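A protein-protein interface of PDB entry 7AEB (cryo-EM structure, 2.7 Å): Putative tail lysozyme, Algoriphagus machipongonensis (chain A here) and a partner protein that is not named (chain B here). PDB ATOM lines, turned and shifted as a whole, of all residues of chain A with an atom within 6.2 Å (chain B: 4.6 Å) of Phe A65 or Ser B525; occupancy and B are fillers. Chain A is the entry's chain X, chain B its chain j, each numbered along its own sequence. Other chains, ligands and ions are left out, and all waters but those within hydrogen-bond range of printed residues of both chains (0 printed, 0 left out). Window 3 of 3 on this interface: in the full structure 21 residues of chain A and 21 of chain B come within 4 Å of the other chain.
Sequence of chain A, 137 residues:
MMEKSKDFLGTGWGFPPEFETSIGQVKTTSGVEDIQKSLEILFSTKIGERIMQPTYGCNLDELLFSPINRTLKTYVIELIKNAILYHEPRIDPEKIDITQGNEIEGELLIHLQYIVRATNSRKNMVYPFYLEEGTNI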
ATOM      1  N   ASP A  61      17.902 -21.867  31.321  1.00  0.00           N
ATOM      2  CA  ASP A  61      19.103 -21.045  31.508  1.00  0.00           C
ATOM      3  C   ASP A  61      20.353 -21.588  30.821  1.00  0.00           C
ATOM      4  O   ASP A  61      21.303 -20.828  30.607  1.00  0.00           O
ATOM      5  CB  ASP A  61      19.465 -20.906  32.977  1.00  0.00           C
ATOM      6  CG  ASP A  61      18.516 -20.054  33.743  1.00  0.00           C
ATOM      7  OD1 ASP A  61      17.703 -19.336  33.161  1.00  0.00           O
ATOM      8  OD2 ASP A  61      18.637 -20.052  34.965  1.00  0.00           O
ATOM      9  N   LEU A  63      20.841 -22.185  27.887  1.00  0.00           N
ATOM     10  CA  LEU A  63      20.962 -21.617  26.572  1.00  0.00           C
ATOM     11  C   LEU A  63      21.321 -20.137  26.579  1.00  0.00           C
ATOM     12  O   LEU A  63      21.340 -19.514  25.514  1.00  0.00           O
ATOM     13  CB  LEU A  63      19.652 -21.859  25.846  1.00  0.00           C
ATOM     14  CG  LEU A  63      19.330 -23.353  25.742  1.00  0.00           C
ATOM     15  CD1 LEU A  63      18.004 -23.487  25.225  1.00  0.00           C
ATOM     16  CD2 LEU A  63      20.324 -24.088  24.856  1.00  0.00           C
ATOM     17  N   LEU A  64      21.604 -19.555  27.735  1.00  0.00           N
ATOM     18  CA  LEU A  64      21.994 -18.154  27.752  1.00  0.00           C
ATOM     19  C   LEU A  64      23.399 -18.019  27.192  1.00  0.00           C
ATOM     20  O   LEU A  64      24.220 -18.920  27.352  1.00  0.00           O
ATOM     21  CB  LEU A  64      21.934 -17.605  29.167  1.00  0.00           C
ATOM     22  CG  LEU A  64      20.547 -17.561  29.800  1.00  0.00           C
ATOM     23  CD1 LEU A  64      20.680 -17.216  31.253  1.00  0.00           C
ATOM     24  CD2 LEU A  64      19.676 -16.539  29.108  1.00  0.00           C
ATOM     25  N   PHE A  65      23.651 -16.898  26.508  1.00  0.00           N
ATOM     26  CA  PHE A  65      24.960 -16.596  25.908  1.00  0.00           C
ATOM     27  C   PHE A  65      25.350 -17.599  24.829  1.00  0.00           C
ATOM     28  O   PHE A  65      26.501 -18.025  24.751  1.00  0.00           O
ATOM     29  CB  PHE A  65      26.077 -16.516  26.956  1.00  0.00           C
ATOM     30  CG  PHE A  65      25.830 -15.527  28.018  1.00  0.00           C
ATOM     31  CD1 PHE A  65      25.343 -15.911  29.248  1.00  0.00           C
ATOM     32  CD2 PHE A  65      26.100 -14.201  27.789  1.00  0.00           C
ATOM     33  CE1 PHE A  65      25.129 -14.983  30.229  1.00  0.00           C
ATOM     34  CE2 PHE A  65      25.888 -13.271  28.764  1.00  0.00           C
ATOM     35  CZ  PHE A  65      25.403 -13.662  29.985  1.00  0.00           C
ATOM     36  N   SER A  66      24.407 -17.950  23.971  1.00  0.00           N
ATOM     37  CA  SER A  66      24.645 -18.888  22.888  1.00  0.00           C
ATOM     38  C   SER A  66      24.013 -18.325  21.621  1.00  0.00           C
ATOM     39  O   SER A  66      23.087 -17.510  21.708  1.00  0.00           O
ATOM     40  CB  SER A  66      24.045 -20.256  23.236  1.00  0.00           C
ATOM     41  OG  SER A  66      22.639 -20.171  23.260  1.00  0.00           O
ATOM     42  N   PRO A  67      24.538 -18.692  20.444  1.00  0.00           N
ATOM     43  CA  PRO A  67      23.955 -18.298  19.149  1.00  0.00           C
ATOM     44  C   PRO A  67      22.670 -19.055  18.874  1.00  0.00           C
ATOM     45  O   PRO A  67      22.459 -20.154  19.383  1.00  0.00           O
ATOM     46  CB  PRO A  67      25.045 -18.715  18.149  1.00  0.00           C
ATOM     47  CG  PRO A  67      25.781 -19.824  18.853  1.00  0.00           C
ATOM     48  CD  PRO A  67      25.783 -19.454  20.285  1.00  0.00           C
ATOM     49  N   VAL B 516      37.258 -21.769  26.240  1.00  0.00           N
ATOM     50  CA  VAL B 516      36.219 -21.447  25.284  1.00  0.00           C
ATOM     51  C   VAL B 516      36.775 -21.405  23.864  1.00  0.00           C
ATOM     52  O   VAL B 516      36.150 -21.930  22.935  1.00  0.00           O
ATOM     53  CB  VAL B 516      35.528 -20.135  25.680  1.00  0.00           C
ATOM     54  CG1 VAL B 516      34.561 -19.671  24.595  1.00  0.00           C
ATOM     55  CG2 VAL B 516      34.785 -20.359  26.982  1.00  0.00           C
ATOM     56  N   TRP B 523      34.749 -16.587  18.613  1.00  0.00           N
ATOM     57  CA  TRP B 523      33.502 -15.853  18.483  1.00  0.00           C
ATOM     58  C   TRP B 523      32.445 -16.264  19.507  1.00  0.00           C
ATOM     59  O   TRP B 523      31.344 -15.711  19.505  1.00  0.00           O
ATOM     60  CB  TRP B 523      32.956 -16.014  17.069  1.00  0.00           C
ATOM     61  CG  TRP B 523      32.853 -17.423  16.621  1.00  0.00           C
ATOM     62  CD1 TRP B 523      31.808 -18.259  16.780  1.00  0.00           C
ATOM     63  CD2 TRP B 523      33.842 -18.155  15.932  1.00  0.00           C
ATOM     64  NE1 TRP B 523      32.083 -19.462  16.231  1.00  0.00           N
ATOM     65  CE2 TRP B 523      33.331 -19.422  15.706  1.00  0.00           C
ATOM     66  CE3 TRP B 523      35.118 -17.852  15.482  1.00  0.00           C
ATOM     67  CZ2 TRP B 523      34.037 -20.384  15.052  1.00  0.00           C
ATOM     68  CZ3 TRP B 523      35.832 -18.809  14.827  1.00  0.00           C
ATOM     69  CH2 TRP B 523      35.301 -20.057  14.617  1.00  0.00           C
ATOM     70  N   LYS B 524      32.752 -17.216  20.372  1.00  0.00           N
ATOM     71  CA  LYS B 524      31.836 -17.656  21.415  1.00  0.00           C
ATOM     72  C   LYS B 524      32.027 -16.840  22.692  1.00  0.00           C
ATOM     73  O   LYS B 524      33.151 -16.644  23.151  1.00  0.00           O
ATOM     74  CB  LYS B 524      32.050 -19.139  21.705  1.00  0.00           C
ATOM     75  CG  LYS B 524      31.312 -19.702  22.925  1.00  0.00           C
ATOM     76  CD  LYS B 524      29.837 -19.881  22.744  1.00  0.00           C
ATOM     77  CE  LYS B 524      29.223 -20.437  24.031  1.00  0.00           C
ATOM     78  NZ  LYS B 524      29.010 -19.384  25.095  1.00  0.00           N
ATOM     79  N   SER B 525      30.935 -16.360  23.262  1.00  0.00           N
ATOM     80  CA  SER B 525      31.006 -15.629  24.524  1.00  0.00           C
ATOM     81  C   SER B 525      31.552 -16.441  25.709  1.00  0.00           C
ATOM     82  O   SER B 525      31.113 -17.574  25.916  1.00  0.00           O
ATOM     83  CB  SER B 525      29.640 -15.122  24.896  1.00  0.00           C
ATOM     84  OG  SER B 525      29.701 -14.472  26.132  1.00  0.00           O
ATOM     85  N   PRO B 526      32.486 -15.863  26.499  1.00  0.00           N
ATOM     86  CA  PRO B 526      33.039 -16.405  27.764  1.00  0.00           C
ATOM     87  C   PRO B 526      32.064 -16.578  28.933  1.00  0.00           C
ATOM     88  O   PRO B 526      32.445 -17.079  29.958  1.00  0.00           O
ATOM     89  CB  PRO B 526      34.080 -15.339  28.142  1.00  0.00           C
ATOM     90  CG  PRO B 526      34.450 -14.676  26.875  1.00  0.00           C
ATOM     91  CD  PRO B 526      33.217 -14.673  26.040  1.00  0.00           C
ATOM     92  N   ALA B 527      30.867 -16.031  28.871  1.00  0.00           N
ATOM     93  CA  ALA B 527      29.932 -16.136  29.988  1.00  0.00           C
ATOM     94  C   ALA B 527      29.311 -17.526  30.120  1.00  0.00           C
ATOM     95  O   ALA B 527      29.306 -18.313  29.177  1.00  0.00           O
ATOM     96  CB  ALA B 527      28.830 -15.112  29.850  1.00  0.00           C
ATOM     97  N   ASN B 528      28.748 -17.780  31.319  1.00  0.00           N
ATOM     98  CA  ASN B 528      28.072 -19.015  31.738  1.00  0.00           C
ATOM     99  C   ASN B 528      29.022 -20.205  31.759  1.00  0.00           C
ATOM    100  O   ASN B 528      28.664 -21.331  31.411  1.00  0.00           O
ATOM    101  CB  ASN B 528      26.856 -19.269  30.861  1.00  0.00           C
ATOM    102  CG  ASN B 528      25.831 -20.185  31.481  1.00  0.00           C
ATOM    103  OD1 ASN B 528      25.716 -20.300  32.699  1.00  0.00           O
ATOM    104  ND2 ASN B 528      25.066 -20.831  30.640  1.00  0.00           N
ATOM    105  N   GLY B 573      27.680 -12.594  32.487  1.00  0.00           N
ATOM    106  CA  GLY B 573      27.868 -11.410  31.658  1.00  0.00           C
ATOM    107  C   GLY B 573      29.217 -11.394  30.940  1.00  0.00           C
ATOM    108  O   GLY B 573      30.212 -11.927  31.433  1.00  0.00           O
ATOM    109  N   ALA B 574      29.246 -10.803  29.745  1.00  0.00           N
ATOM    110  CA  ALA B 574      30.469 -10.744  28.946  1.00  0.00           C
ATOM    111  C   ALA B 574      30.575  -9.484  28.099  1.00  0.00           C
ATOM    112  O   ALA B 574      30.717  -9.565  26.871  1.00  0.00           O
ATOM    113  CB  ALA B 574      30.592 -11.961  28.044  1.00  0.00           C
ATOM    114  N   SER B 588      33.315 -11.035  22.716  1.00  0.00           N
ATOM    115  CA  SER B 588      33.532 -11.957  21.606  1.00  0.00           C
ATOM    116  C   SER B 588      33.569 -11.276  20.253  1.00  0.00           C
ATOM    117  O   SER B 588      34.303 -11.709  19.362  1.00  0.00           O
ATOM    118  CB  SER B 588      32.443 -13.001  21.599  1.00  0.00           C
ATOM    119  OG  SER B 588      31.192 -12.415  21.348  1.00  0.00           O
ATOM    120  N   PRO B 677      25.496 -12.754  20.474  1.00  0.00           N
ATOM    121  CA  PRO B 677      24.853 -13.655  21.453  1.00  0.00           C
ATOM    122  C   PRO B 677      23.463 -13.254  21.923  1.00  0.00           C
ATOM    123  O   PRO B 677      23.101 -12.084  21.921  1.00  0.00           O
ATOM    124  CB  PRO B 677      25.805 -13.549  22.644  1.00  0.00           C
ATOM    125  CG  PRO B 677      26.379 -12.172  22.531  1.00  0.00           C
ATOM    126  CD  PRO B 677      26.543 -11.928  21.074  1.00  0.00           C
ATOM    127  N   ALA B 678      22.707 -14.236  22.408  1.00  0.00           N
ATOM    128  CA  ALA B 678      21.447 -13.940  23.078  1.00  0.00           C
ATOM    129  C   ALA B 678      21.681 -13.744  24.570  1.00  0.00           C
ATOM    130  O   ALA B 678      22.331 -14.572  25.202  1.00  0.00           O
ATOM    131  CB  ALA B 678      20.451 -15.063  22.870  1.00  0.00           C
ATOM    132  N   GLU B 679      21.113 -12.684  25.140  1.00  0.00           N
ATOM    133  CA  GLU B 679      21.230 -12.437  26.574  1.00  0.00           C
ATOM    134  C   GLU B 679      19.919 -12.590  27.329  1.00  0.00           C
ATOM    135  O   GLU B 679      19.938 -12.831  28.536  1.00  0.00           O
ATOM    136  CB  GLU B 679      21.794 -11.035  26.847  1.00  0.00           C
ATOM    137  CG  GLU B 679      23.243 -10.822  26.438  1.00  0.00           C
ATOM    138  CD  GLU B 679      23.742  -9.402  26.714  1.00  0.00           C
ATOM    139  OE1 GLU B 679      23.272  -8.489  26.060  1.00  0.00           O
ATOM    140  OE2 GLU B 679      24.614  -9.211  27.547  1.00  0.00           O
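The backbone carbonyl oxygen (O) of Phe A65 lies within hydrogen-bond range of the side-chain amino group (NZ) of Lys B524 (2.9 Å). The backbone NH of Phe A65 lies within hydrogen-bond range of the backbone carbonyl oxygen of Ala B678 (3.0 Å). The backbone carbonyl oxygen (O) of Ser A66 is in hydrogen-bond range of the backbone NH (N) of Ala B678, 3.4 Å away.
The backbone NH (N) of Ala B527 sits close to the side-chain hydroxyl (OG) of Ser B525. The side-chain hydroxyl (OG) of Ser A66 lies within hydrogen-bond range of the backbone carbonyl oxygen (O) of Leu A63 (2.7 Å).
Among the printed residues, pairs that only touch across the chains: Asp A61 with Asn B528 (3.8 Å), Leu A64 with Asn B528 (3.9 Å), Leu A64 with Glu B679 (3.8 Å), Phe A65 with Ser B525 (3.97 Å), Phe A65 with Ala B527 (3.5 Å) and Phe A65 with Gly B573 (3.5 Å).
Of chain B, only Lys B524 (2.9 Å), Ser B525 (3.97 Å), Ala B527 (3.5 Å), Gly B573 (3.5 Å) and Ala B678 (3.0 Å) come within 4 Å of Phe A65. Ser B525 touches one residue of chain A. Printed residues of chain B within 4 Å of Leu A64: Asn B528 (3.9 Å) and Glu B679 (3.8 Å). Printed residues of chain A within 4 Å of Ala B678: Phe A65 and Ser A66. Ala B574 touches none of the printed residues of chain A. Pro B677 touches none of the printed residues of chain A. The nearest residue of chain B that does not touch Phe A65 is Asn B528 (4.02 Å). The nearest printed residue of chain B that does not touch Asp A61 is Glu B679 (8.3 Å).
Of the 6 printed residues of chain A, 4 touch a printed residue of chain B. Of the 13 printed residues of chain B, 7 touch a printed residue of chain A. Hydrophobic or aromatic side chains of chain B within 4 Å of the printed part of chain A: Ala B527 and Ala B678.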
